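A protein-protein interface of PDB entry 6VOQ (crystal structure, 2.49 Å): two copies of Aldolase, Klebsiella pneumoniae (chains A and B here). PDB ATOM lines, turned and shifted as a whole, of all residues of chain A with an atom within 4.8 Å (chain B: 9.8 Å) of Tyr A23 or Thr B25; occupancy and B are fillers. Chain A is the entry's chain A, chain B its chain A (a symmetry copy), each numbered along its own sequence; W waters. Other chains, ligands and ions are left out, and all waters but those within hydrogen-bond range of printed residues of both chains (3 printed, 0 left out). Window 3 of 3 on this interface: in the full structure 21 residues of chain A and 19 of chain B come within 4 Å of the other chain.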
ATOM      1  N   LEU A  18      -3.880 -11.302  15.159  1.00  0.00           N
ATOM      2  CA  LEU A  18      -2.913 -10.996  16.206  1.00  0.00           C
ATOM      3  C   LEU A  18      -3.614 -10.572  17.490  1.00  0.00           C
ATOM      4  O   LEU A  18      -3.181 -10.937  18.590  1.00  0.00           O
ATOM      5  CB  LEU A  18      -1.957  -9.899  15.736  1.00  0.00           C
ATOM      6  CG  LEU A  18      -1.028 -10.242  14.576  1.00  0.00           C
ATOM      7  CD1 LEU A  18      -0.356  -8.981  14.064  1.00  0.00           C
ATOM      8  CD2 LEU A  18       0.002 -11.286  14.989  1.00  0.00           C
ATOM      9  N   ARG A  21      -5.501 -13.553  19.333  1.00  0.00           N
ATOM     10  CA  ARG A  21      -4.603 -14.562  19.876  1.00  0.00           C
ATOM     11  C   ARG A  21      -3.600 -13.998  20.871  1.00  0.00           C
ATOM     12  O   ARG A  21      -2.691 -14.714  21.287  1.00  0.00           O
ATOM     13  CB  ARG A  21      -3.888 -15.295  18.744  1.00  0.00           C
ATOM     14  CG  ARG A  21      -4.809 -16.249  17.994  1.00  0.00           C
ATOM     15  CD  ARG A  21      -4.121 -16.870  16.805  1.00  0.00           C
ATOM     16  NE  ARG A  21      -3.505 -15.862  15.945  1.00  0.00           N
ATOM     17  CZ  ARG A  21      -2.256 -15.934  15.498  1.00  0.00           C
ATOM     18  NH1 ARG A  21      -1.496 -16.975  15.819  1.00  0.00           N
ATOM     19  NH2 ARG A  21      -1.769 -14.977  14.720  1.00  0.00           N
ATOM     20  N   GLY A  22      -3.757 -12.744  21.283  1.00  0.00           N
ATOM     21  CA  GLY A  22      -3.022 -12.224  22.416  1.00  0.00           C
ATOM     22  C   GLY A  22      -1.709 -11.551  22.090  1.00  0.00           C
ATOM     23  O   GLY A  22      -1.071 -11.014  23.002  1.00  0.00           O
ATOM     24  N   TYR A  23      -1.282 -11.566  20.823  1.00  0.00           N
ATOM     25  CA  TYR A  23      -0.047 -10.894  20.432  1.00  0.00           C
ATOM     26  C   TYR A  23      -0.157  -9.383  20.575  1.00  0.00           C
ATOM     27  O   TYR A  23       0.856  -8.711  20.797  1.00  0.00           O
ATOM     28  CB  TYR A  23       0.314 -11.248  18.992  1.00  0.00           C
ATOM     29  CG  TYR A  23       0.695 -12.682  18.801  1.00  0.00           C
ATOM     30  CD1 TYR A  23      -0.264 -13.634  18.453  1.00  0.00           C
ATOM     31  CD2 TYR A  23       2.013 -13.096  18.968  1.00  0.00           C
ATOM     32  CE1 TYR A  23       0.076 -14.960  18.277  1.00  0.00           C
ATOM     33  CE2 TYR A  23       2.364 -14.422  18.804  1.00  0.00           C
ATOM     34  CZ  TYR A  23       1.390 -15.352  18.456  1.00  0.00           C
ATOM     35  OH  TYR A  23       1.729 -16.675  18.283  1.00  0.00           O
ATOM     36  N   ALA A  24      -1.358  -8.827  20.429  1.00  0.00           N
ATOM     37  CA  ALA A  24      -1.588  -7.404  20.640  1.00  0.00           C
ATOM     38  C   ALA A  24      -2.707  -7.221  21.649  1.00  0.00           C
ATOM     39  O   ALA A  24      -3.722  -7.925  21.600  1.00  0.00           O
ATOM     40  CB  ALA A  24      -1.942  -6.671  19.340  1.00  0.00           C
ATOM     41  N   THR A  25      -2.510  -6.278  22.566  1.00  0.00           N
ATOM     42  CA  THR A  25      -3.509  -5.942  23.569  1.00  0.00           C
ATOM     43  C   THR A  25      -3.761  -4.444  23.548  1.00  0.00           C
ATOM     44  O   THR A  25      -2.827  -3.654  23.403  1.00  0.00           O
ATOM     45  CB  THR A  25      -3.066  -6.350  24.976  1.00  0.00           C
ATOM     46  OG1 THR A  25      -2.076  -5.424  25.440  1.00  0.00           O
ATOM     47  CG2 THR A  25      -2.491  -7.764  24.983  1.00  0.00           C
ATOM     48  N   LEU A  95       4.863  -4.984  17.457  1.00  0.00           N
ATOM     49  CA  LEU A  95       3.982  -5.394  18.536  1.00  0.00           C
ATOM     50  C   LEU A  95       4.688  -5.182  19.862  1.00  0.00           C
ATOM     51  O   LEU A  95       5.911  -5.070  19.924  1.00  0.00           O
ATOM     52  CB  LEU A  95       3.588  -6.867  18.419  1.00  0.00           C
ATOM     53  CG  LEU A  95       2.804  -7.300  17.201  1.00  0.00           C
ATOM     54  CD1 LEU A  95       2.811  -8.803  17.191  1.00  0.00           C
ATOM     55  CD2 LEU A  95       1.391  -6.755  17.275  1.00  0.00           C
ATOM     56  N   HIS A  96       3.899  -5.122  20.927  1.00  0.00           N
ATOM     57  CA  HIS A  96       4.432  -5.277  22.275  1.00  0.00           C
ATOM     58  C   HIS A  96       4.176  -6.685  22.776  1.00  0.00           C
ATOM     59  O   HIS A  96       3.680  -6.870  23.894  1.00  0.00           O
ATOM     60  CB  HIS A  96       3.835  -4.240  23.222  1.00  0.00           C
ATOM     61  CG  HIS A  96       4.019  -2.828  22.764  1.00  0.00           C
ATOM     62  ND1 HIS A  96       3.515  -1.750  23.459  1.00  0.00           N
ATOM     63  CD2 HIS A  96       4.647  -2.316  21.681  1.00  0.00           C
ATOM     64  CE1 HIS A  96       3.816  -0.635  22.820  1.00  0.00           C
ATOM     65  NE2 HIS A  96       4.503  -0.951  21.737  1.00  0.00           N
ATOM     66  N   SER A  97       4.471  -7.690  21.947  1.00  0.00           N
ATOM     67  CA  SER A  97       4.161  -9.064  22.321  1.00  0.00           C
ATOM     68  C   SER A  97       4.941  -9.431  23.579  1.00  0.00           C
ATOM     69  O   SER A  97       6.063  -8.961  23.795  1.00  0.00           O
ATOM     70  CB  SER A  97       4.455 -10.029  21.162  1.00  0.00           C
ATOM     71  OG  SER A  97       5.807  -9.971  20.716  1.00  0.00           O
ATOM     72  N   GLU A 178       5.729 -14.085  14.865  1.00  0.00           N
ATOM     73  CA  GLU A 178       5.226 -15.165  15.698  1.00  0.00           C
ATOM     74  C   GLU A 178       6.338 -16.140  16.046  1.00  0.00           C
ATOM     75  O   GLU A 178       6.391 -16.643  17.171  1.00  0.00           O
ATOM     76  CB  GLU A 178       4.074 -15.878  15.001  1.00  0.00           C
ATOM     77  CG  GLU A 178       2.797 -15.094  15.036  1.00  0.00           C
ATOM     78  CD  GLU A 178       1.779 -15.625  14.075  1.00  0.00           C
ATOM     79  OE1 GLU A 178       2.140 -15.869  12.914  1.00  0.00           O
ATOM     80  OE2 GLU A 178       0.617 -15.802  14.478  1.00  0.00           O
ATOM     81  N   GLU A 181       8.439 -14.348  18.742  1.00  0.00           N
ATOM     82  CA  GLU A 181       7.779 -14.301  20.040  1.00  0.00           C
ATOM     83  C   GLU A 181       7.802 -15.667  20.706  1.00  0.00           C
ATOM     84  O   GLU A 181       8.078 -15.779  21.906  1.00  0.00           O
ATOM     85  CB  GLU A 181       6.350 -13.787  19.876  1.00  0.00           C
ATOM     86  CG  GLU A 181       5.469 -13.955  21.104  1.00  0.00           C
ATOM     87  CD  GLU A 181       5.832 -13.025  22.262  1.00  0.00           C
ATOM     88  OE1 GLU A 181       6.672 -12.111  22.100  1.00  0.00           O
ATOM     89  OE2 GLU A 181       5.255 -13.211  23.348  1.00  0.00           O
ATOM     90  N   GLU A 182       7.552 -16.718  19.925  1.00  0.00           N
ATOM     91  CA  GLU A 182       7.620 -18.081  20.432  1.00  0.00           C
ATOM     92  C   GLU A 182       9.017 -18.419  20.936  1.00  0.00           C
ATOM     93  O   GLU A 182       9.173 -19.124  21.940  1.00  0.00           O
ATOM     94  CB  GLU A 182       7.192 -19.044  19.329  1.00  0.00           C
ATOM     95  CG  GLU A 182       7.280 -20.485  19.702  1.00  0.00           C
ATOM     96  CD  GLU A 182       6.334 -20.847  20.826  1.00  0.00           C
ATOM     97  OE1 GLU A 182       6.642 -21.819  21.543  1.00  0.00           O
ATOM     98  OE2 GLU A 182       5.298 -20.162  20.993  1.00  0.00           O
ATOM     99  N   GLY B  15      -6.841 -28.410  11.954  1.00  0.00           N
ATOM    100  CA  GLY B  15      -5.852 -27.347  11.828  1.00  0.00           C
ATOM    101  C   GLY B  15      -6.318 -26.037  12.437  1.00  0.00           C
ATOM    102  O   GLY B  15      -5.602 -25.419  13.227  1.00  0.00           O
ATOM    103  N   ALA B  16      -7.537 -25.613  12.102  1.00  0.00           N
ATOM    104  CA  ALA B  16      -8.070 -24.358  12.627  1.00  0.00           C
ATOM    105  C   ALA B  16      -8.189 -24.397  14.148  1.00  0.00           C
ATOM    106  O   ALA B  16      -7.892 -23.406  14.824  1.00  0.00           O
ATOM    107  CB  ALA B  16      -9.433 -24.063  11.988  1.00  0.00           C
ATOM    108  N   SER B  17      -8.628 -25.534  14.697  1.00  0.00           N
ATOM    109  CA  SER B  17      -8.767 -25.678  16.144  1.00  0.00           C
ATOM    110  C   SER B  17      -7.417 -25.590  16.838  1.00  0.00           C
ATOM    111  O   SER B  17      -7.298 -24.974  17.904  1.00  0.00           O
ATOM    112  CB  SER B  17      -9.450 -27.009  16.469  1.00  0.00           C
ATOM    113  OG  SER B  17      -9.796 -27.102  17.837  1.00  0.00           O
ATOM    114  N   LEU B  18      -6.389 -26.194  16.239  1.00  0.00           N
ATOM    115  CA  LEU B  18      -5.050 -26.129  16.813  1.00  0.00           C
ATOM    116  C   LEU B  18      -4.480 -24.720  16.709  1.00  0.00           C
ATOM    117  O   LEU B  18      -3.811 -24.245  17.635  1.00  0.00           O
ATOM    118  CB  LEU B  18      -4.128 -27.128  16.115  1.00  0.00           C
ATOM    119  CG  LEU B  18      -4.447 -28.609  16.296  1.00  0.00           C
ATOM    120  CD1 LEU B  18      -3.620 -29.437  15.331  1.00  0.00           C
ATOM    121  CD2 LEU B  18      -4.215 -29.046  17.736  1.00  0.00           C
ATOM    122  N   PHE B  19      -4.739 -24.033  15.594  1.00  0.00           N
ATOM    123  CA  PHE B  19      -4.195 -22.692  15.417  1.00  0.00           C
ATOM    124  C   PHE B  19      -4.877 -21.693  16.337  1.00  0.00           C
ATOM    125  O   PHE B  19      -4.206 -20.887  16.993  1.00  0.00           O
ATOM    126  CB  PHE B  19      -4.340 -22.244  13.967  1.00  0.00           C
ATOM    127  CG  PHE B  19      -3.651 -20.939  13.661  1.00  0.00           C
ATOM    128  CD1 PHE B  19      -2.301 -20.911  13.316  1.00  0.00           C
ATOM    129  CD2 PHE B  19      -4.347 -19.744  13.700  1.00  0.00           C
ATOM    130  CE1 PHE B  19      -1.664 -19.713  13.013  1.00  0.00           C
ATOM    131  CE2 PHE B  19      -3.715 -18.545  13.402  1.00  0.00           C
ATOM    132  CZ  PHE B  19      -2.372 -18.531  13.057  1.00  0.00           C
ATOM    133  N   SER B  20      -6.207 -21.723  16.398  1.00  0.00           N
ATOM    134  CA  SER B  20      -6.903 -20.731  17.209  1.00  0.00           C
ATOM    135  C   SER B  20      -6.587 -20.892  18.689  1.00  0.00           C
ATOM    136  O   SER B  20      -6.631 -19.910  19.438  1.00  0.00           O
ATOM    137  CB  SER B  20      -8.411 -20.815  16.971  1.00  0.00           C
ATOM    138  OG  SER B  20      -8.917 -22.057  17.420  1.00  0.00           O
ATOM    139  N   ARG B  21      -6.251 -22.103  19.130  1.00  0.00           N
ATOM    140  CA  ARG B  21      -6.001 -22.356  20.542  1.00  0.00           C
ATOM    141  C   ARG B  21      -4.521 -22.351  20.899  1.00  0.00           C
ATOM    142  O   ARG B  21      -4.168 -22.699  22.024  1.00  0.00           O
ATOM    143  CB  ARG B  21      -6.655 -23.669  20.966  1.00  0.00           C
ATOM    144  CG  ARG B  21      -8.171 -23.560  21.062  1.00  0.00           C
ATOM    145  CD  ARG B  21      -8.808 -24.893  21.360  1.00  0.00           C
ATOM    146  NE  ARG B  21      -8.358 -25.930  20.435  1.00  0.00           N
ATOM    147  CZ  ARG B  21      -7.927 -27.128  20.818  1.00  0.00           C
ATOM    148  NH1 ARG B  21      -7.903 -27.441  22.109  1.00  0.00           N
ATOM    149  NH2 ARG B  21      -7.535 -28.016  19.916  1.00  0.00           N
ATOM    150  N   GLY B  22      -3.653 -21.939  19.981  1.00  0.00           N
ATOM    151  CA  GLY B  22      -2.277 -21.647  20.321  1.00  0.00           C
ATOM    152  C   GLY B  22      -1.309 -22.798  20.173  1.00  0.00           C
ATOM    153  O   GLY B  22      -0.105 -22.595  20.369  1.00  0.00           O
ATOM    154  N   TYR B  23      -1.793 -23.999  19.838  1.00  0.00           N
ATOM    155  CA  TYR B  23      -0.908 -25.141  19.632  1.00  0.00           C
ATOM    156  C   TYR B  23      -0.016 -24.952  18.414  1.00  0.00           C
ATOM    157  O   TYR B  23       1.089 -25.503  18.369  1.00  0.00           O
ATOM    158  CB  TYR B  23      -1.725 -26.421  19.477  1.00  0.00           C
ATOM    159  CG  TYR B  23      -2.441 -26.835  20.723  1.00  0.00           C
ATOM    160  CD1 TYR B  23      -3.749 -26.413  20.966  1.00  0.00           C
ATOM    161  CD2 TYR B  23      -1.817 -27.646  21.666  1.00  0.00           C
ATOM    162  CE1 TYR B  23      -4.418 -26.786  22.115  1.00  0.00           C
ATOM    163  CE2 TYR B  23      -2.473 -28.018  22.823  1.00  0.00           C
ATOM    164  CZ  TYR B  23      -3.778 -27.587  23.043  1.00  0.00           C
ATOM    165  OH  TYR B  23      -4.443 -27.958  24.189  1.00  0.00           O
ATOM    166  N   ALA B  24      -0.478 -24.207  17.411  1.00  0.00           N
ATOM    167  CA  ALA B  24       0.331 -23.886  16.244  1.00  0.00           C
ATOM    168  C   ALA B  24       0.361 -22.380  16.053  1.00  0.00           C
ATOM    169  O   ALA B  24      -0.665 -21.706  16.194  1.00  0.00           O
ATOM    170  CB  ALA B  24      -0.194 -24.556  14.967  1.00  0.00           C
ATOM    171  N   THR B  25       1.546 -21.861  15.740  1.00  0.00           N
ATOM    172  CA  THR B  25       1.731 -20.443  15.471  1.00  0.00           C
ATOM    173  C   THR B  25       2.438 -20.271  14.138  1.00  0.00           C
ATOM    174  O   THR B  25       3.356 -21.026  13.814  1.00  0.00           O
ATOM    175  CB  THR B  25       2.557 -19.758  16.562  1.00  0.00           C
ATOM    176  OG1 THR B  25       3.934 -20.118  16.401  1.00  0.00           O
ATOM    177  CG2 THR B  25       2.078 -20.167  17.954  1.00  0.00           C
ATOM    178  N   GLY B  26       2.005 -19.278  13.373  1.00  0.00           N
ATOM    179  CA  GLY B  26       2.721 -18.927  12.157  1.00  0.00           C
ATOM    180  C   GLY B  26       2.671 -20.041  11.133  1.00  0.00           C
ATOM    181  O   GLY B  26       1.616 -20.621  10.860  1.00  0.00           O
ATOM    182  N   SER B  27       3.831 -20.348  10.560  1.00  0.00           N
ATOM    183  CA  SER B  27       3.968 -21.358   9.521  1.00  0.00           C
ATOM    184  C   SER B  27       4.297 -22.743  10.068  1.00  0.00           C
ATOM    185  O   SER B  27       4.547 -23.657   9.278  1.00  0.00           O
ATOM    186  CB  SER B  27       5.051 -20.926   8.526  1.00  0.00           C
ATOM    187  OG  SER B  27       6.352 -21.172   9.043  1.00  0.00           O
ATOM    188  N   ALA B  28       4.302 -22.923  11.388  1.00  0.00           N
ATOM    189  CA  ALA B  28       4.799 -24.154  11.993  1.00  0.00           C
ATOM    190  C   ALA B  28       3.717 -25.222  12.081  1.00  0.00           C
ATOM    191  O   ALA B  28       2.551 -24.932  12.369  1.00  0.00           O
ATOM    192  CB  ALA B  28       5.360 -23.888  13.388  1.00  0.00           C
ATOM    193  N   GLY B  29       4.119 -26.459  11.842  1.00  0.00           N
ATOM    194  CA  GLY B  29       3.254 -27.597  12.061  1.00  0.00           C
ATOM    195  C   GLY B  29       2.743 -28.185  10.763  1.00  0.00           C
ATOM    196  O   GLY B  29       2.656 -27.515   9.729  1.00  0.00           O
ATOM    197  N   ASN B  30       2.402 -29.467  10.813  1.00  0.00           N
ATOM    198  CA  ASN B  30       1.796 -30.130   9.671  1.00  0.00           C
ATOM    199  C   ASN B  30       1.013 -31.343  10.157  1.00  0.00           C
ATOM    200  O   ASN B  30       1.277 -31.884  11.232  1.00  0.00           O
ATOM    201  CB  ASN B  30       2.846 -30.528   8.634  1.00  0.00           C
ATOM    202  CG  ASN B  30       4.109 -31.052   9.263  1.00  0.00           C
ATOM    203  OD1 ASN B  30       4.186 -32.215   9.648  1.00  0.00           O
ATOM    204  ND2 ASN B  30       5.115 -30.193   9.372  1.00  0.00           N
ATOM    205  N   ALA B  47       2.300 -23.703   4.538  1.00  0.00           N
ATOM    206  CA  ALA B  47       0.906 -23.524   4.906  1.00  0.00           C
ATOM    207  C   ALA B  47       0.782 -23.067   6.351  1.00  0.00           C
ATOM    208  O   ALA B  47       1.692 -23.236   7.170  1.00  0.00           O
ATOM    209  CB  ALA B  47       0.125 -24.822   4.703  1.00  0.00           C
ATOM    210  N   CYS B  48      -0.370 -22.479   6.650  1.00  0.00           N
ATOM    211  CA  CYS B  48      -0.732 -22.056   7.994  1.00  0.00           C
ATOM    212  C   CYS B  48      -1.950 -22.864   8.421  1.00  0.00           C
ATOM    213  O   CYS B  48      -2.982 -22.845   7.740  1.00  0.00           O
ATOM    214  CB  CYS B  48      -1.016 -20.548   8.032  1.00  0.00           C
ATOM    215  SG  CYS B  48      -1.836 -19.937   9.520  1.00  0.00           S
ATOM    216  N   LEU B  49      -1.821 -23.593   9.533  1.00  0.00           N
ATOM    217  CA  LEU B  49      -2.861 -24.534   9.936  1.00  0.00           C
ATOM    218  C   LEU B  49      -4.221 -23.875  10.119  1.00  0.00           C
ATOM    219  O   LEU B  49      -5.242 -24.564  10.039  1.00  0.00           O
ATOM    220  CB  LEU B  49      -2.458 -25.237  11.226  1.00  0.00           C
ATOM    221  CG  LEU B  49      -1.270 -26.178  11.046  1.00  0.00           C
ATOM    222  CD1 LEU B  49      -1.050 -26.998  12.301  1.00  0.00           C
ATOM    223  CD2 LEU B  49      -1.504 -27.073   9.845  1.00  0.00           C
ATOM    224  N   GLY B  50      -4.262 -22.574  10.372  1.00  0.00           N
ATOM    225  CA  GLY B  50      -5.539 -21.907  10.454  1.00  0.00           C
ATOM    226  C   GLY B  50      -6.115 -21.454   9.136  1.00  0.00           C
ATOM    227  O   GLY B  50      -7.195 -20.864   9.125  1.00  0.00           O
ATOM    228  N   HIS B  94       2.195 -33.165  13.770  1.00  0.00           N
ATOM    229  CA  HIS B  94       3.475 -32.570  14.108  1.00  0.00           C
ATOM    230  C   HIS B  94       3.260 -31.096  14.404  1.00  0.00           C
ATOM    231  O   HIS B  94       2.721 -30.363  13.569  1.00  0.00           O
ATOM    232  CB  HIS B  94       4.494 -32.735  12.993  1.00  0.00           C
ATOM    233  CG  HIS B  94       5.736 -31.936  13.221  1.00  0.00           C
ATOM    234  ND1 HIS B  94       6.516 -32.086  14.349  1.00  0.00           N
ATOM    235  CD2 HIS B  94       6.315 -30.956  12.490  1.00  0.00           C
ATOM    236  CE1 HIS B  94       7.535 -31.249  14.290  1.00  0.00           C
ATOM    237  NE2 HIS B  94       7.435 -30.550  13.173  1.00  0.00           N
ATOM    238  N   LEU B  95       3.670 -30.670  15.587  1.00  0.00           N
ATOM    239  CA  LEU B  95       3.536 -29.286  16.006  1.00  0.00           C
ATOM    240  C   LEU B  95       4.827 -28.839  16.666  1.00  0.00           C
ATOM    241  O   LEU B  95       5.640 -29.655  17.097  1.00  0.00           O
ATOM    242  CB  LEU B  95       2.388 -29.102  17.000  1.00  0.00           C
ATOM    243  CG  LEU B  95       0.986 -29.419  16.534  1.00  0.00           C
ATOM    244  CD1 LEU B  95       0.115 -29.441  17.758  1.00  0.00           C
ATOM    245  CD2 LEU B  95       0.520 -28.369  15.544  1.00  0.00           C
ATOM    246  N   HIS B  96       5.011 -27.526  16.732  1.00  0.00           N
ATOM    247  CA  HIS B  96       6.002 -26.945  17.630  1.00  0.00           C
ATOM    248  C   HIS B  96       5.325 -26.418  18.880  1.00  0.00           C
ATOM    249  O   HIS B  96       5.568 -25.276  19.288  1.00  0.00           O
ATOM    250  CB  HIS B  96       6.795 -25.845  16.930  1.00  0.00           C
ATOM    251  CG  HIS B  96       7.457 -26.291  15.665  1.00  0.00           C
ATOM    252  ND1 HIS B  96       8.183 -25.435  14.866  1.00  0.00           N
ATOM    253  CD2 HIS B  96       7.500 -27.498  15.057  1.00  0.00           C
ATOM    254  CE1 HIS B  96       8.639 -26.093  13.816  1.00  0.00           C
ATOM    255  NE2 HIS B  96       8.238 -27.348  13.908  1.00  0.00           N
ATOM    256  N   SER B  97       4.442 -27.221  19.480  1.00  0.00           N
ATOM    257  CA  SER B  97       3.680 -26.747  20.628  1.00  0.00           C
ATOM    258  C   SER B  97       4.642 -26.404  21.761  1.00  0.00           C
ATOM    259  O   SER B  97       5.690 -27.038  21.923  1.00  0.00           O
ATOM    260  CB  SER B  97       2.632 -27.784  21.059  1.00  0.00           C
ATOM    261  OG  SER B  97       3.198 -29.052  21.379  1.00  0.00           O
ATOM    262  N   HIS B  98       4.294 -25.365  22.522  1.00  0.00           N
ATOM    263  CA  HIS B  98       5.308 -24.612  23.253  1.00  0.00           C
ATOM    264  C   HIS B  98       6.058 -25.487  24.253  1.00  0.00           C
ATOM    265  O   HIS B  98       7.294 -25.558  24.238  1.00  0.00           O
ATOM    266  CB  HIS B  98       4.681 -23.418  23.962  1.00  0.00           C
ATOM    267  CG  HIS B  98       5.669 -22.652  24.773  1.00  0.00           C
ATOM    268  ND1 HIS B  98       6.614 -21.823  24.204  1.00  0.00           N
ATOM    269  CD2 HIS B  98       5.933 -22.671  26.103  1.00  0.00           C
ATOM    270  CE1 HIS B  98       7.382 -21.321  25.155  1.00  0.00           C
ATOM    271  NE2 HIS B  98       6.992 -21.821  26.315  1.00  0.00           N
ATOM    272  N   THR B 101       8.006 -28.443  22.791  1.00  0.00           N
ATOM    273  CA  THR B 101       9.215 -27.913  22.171  1.00  0.00           C
ATOM    274  C   THR B 101      10.232 -27.497  23.227  1.00  0.00           C
ATOM    275  O   THR B 101      11.435 -27.738  23.068  1.00  0.00           O
ATOM    276  CB  THR B 101       8.877 -26.713  21.276  1.00  0.00           C
ATOM    277  OG1 THR B 101       8.003 -27.116  20.216  1.00  0.00           O
ATOM    278  CG2 THR B 101      10.145 -26.092  20.680  1.00  0.00           C
ATOM    279  N   GLU B 181       1.073 -32.336  25.211  1.00  0.00           N
ATOM    280  CA  GLU B 181       1.458 -30.949  25.437  1.00  0.00           C
ATOM    281  C   GLU B 181       1.061 -30.500  26.834  1.00  0.00           C
ATOM    282  O   GLU B 181       1.842 -29.843  27.531  1.00  0.00           O
ATOM    283  CB  GLU B 181       0.828 -30.056  24.369  1.00  0.00           C
ATOM    284  CG  GLU B 181       0.919 -28.565  24.651  1.00  0.00           C
ATOM    285  CD  GLU B 181       2.330 -27.992  24.516  1.00  0.00           C
ATOM    286  OE1 GLU B 181       3.255 -28.691  24.045  1.00  0.00           O
ATOM    287  OE2 GLU B 181       2.507 -26.815  24.879  1.00  0.00           O
HETATM  288  O   HOH W   1       3.596 -23.026  20.004  1.00  0.00           O
HETATM  289  O   HOH W   2      -1.781 -19.291  17.353  1.00  0.00           O
HETATM  290  O   HOH W   3       7.583 -23.658  19.976  1.00  0.00           O
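The side-chain carboxylate (OE1) of Glu A178 lies close to the backbone NH (N) of Gly B26. ND1 of His B98 lies within hydrogen-bond range of OE1 of Glu A182.
The backbone carbonyl oxygen (O) of Leu A18 sits at hydrogen-bond distance from the backbone NH (N) of Tyr A23 (3.0 Å). OE2 of Glu A178 is in salt-bridge range of NH2 of Arg A21 (2.5 Å). The backbone carbonyl oxygen of Gly B26 sits at hydrogen-bond distance from the side-chain sulfur of Cys B48 (3.8 Å). The backbone NH (N) of His B98 is in hydrogen-bond range of the side-chain carboxylate (OE2) of Glu B181, 3.3 Å away.
CZ of Phe B19 touches NH1 of Arg A21, at 3.3 Å. Tyr A23 touches Thr B25.
Tyr A23 touches one residue of chain B. Of chain A, only Tyr A23 (3.5 Å) comes within 4 Å of Thr B25. Of chain B, only Phe B19 (3.3 Å) comes within 4 Å of Arg A21. No residue of chain B comes within 4 Å of Ala A24. Glu A178 touches just one residue of chain B: Gly B26 (3.2 Å). Of the printed residues of chain A, Gly B26 touches Glu A178 (3.2 Å). Printed residues of chain A within 4 Å of His B98: Glu A182 (2.7 Å). Of the printed residues of chain B, Glu A182 touches His B98. Of the printed residues of chain A, Phe B19 touches Arg A21 (3.3 Å). Cys B48 touches none of the printed residues of chain A.
Hydrophobic or aromatic side chains of chain A within 4 Å of the printed part of chain B: Tyr A23. Printed residues of chain B that touch a printed residue of chain A: Phe B19, Thr B25, Gly B26 and His B98. Hydrophobic or aromatic side chains of chain B that line the printed part of chain A: Phe B19 and His B98. Along chain B the printed residues that touch a printed residue of chain A span positions 19 to 98. Among the printed residues, 4 pairs touch across the chains. Among the printed residues, no Asp or Glu carboxylate lies within 4 Å of a Lys or Arg side-chain nitrogen of the other chain.
Tyr A23 touches Thr B25, but with the chains exchanged Thr A25 does not touch Tyr B23 (17.0 Å).
Water W3 lies within hydrogen-bond range of OE1 of Glu A182 (2.6 Å), O of His B96 (2.7 Å) and OG1 of Thr B101 (3.5 Å). Water W2 lies within hydrogen-bond range of the guanidinium group of Arg A21, the backbone carbonyl oxygen of Ala B24 and the backbone carbonyl oxygen of Phe B19. Water W1 lies within hydrogen-bond range of the backbone carbonyl oxygen (O) of His B96 (3.1 Å) and the side-chain carboxylate (OE2) of Glu A182 (3.5 Å).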
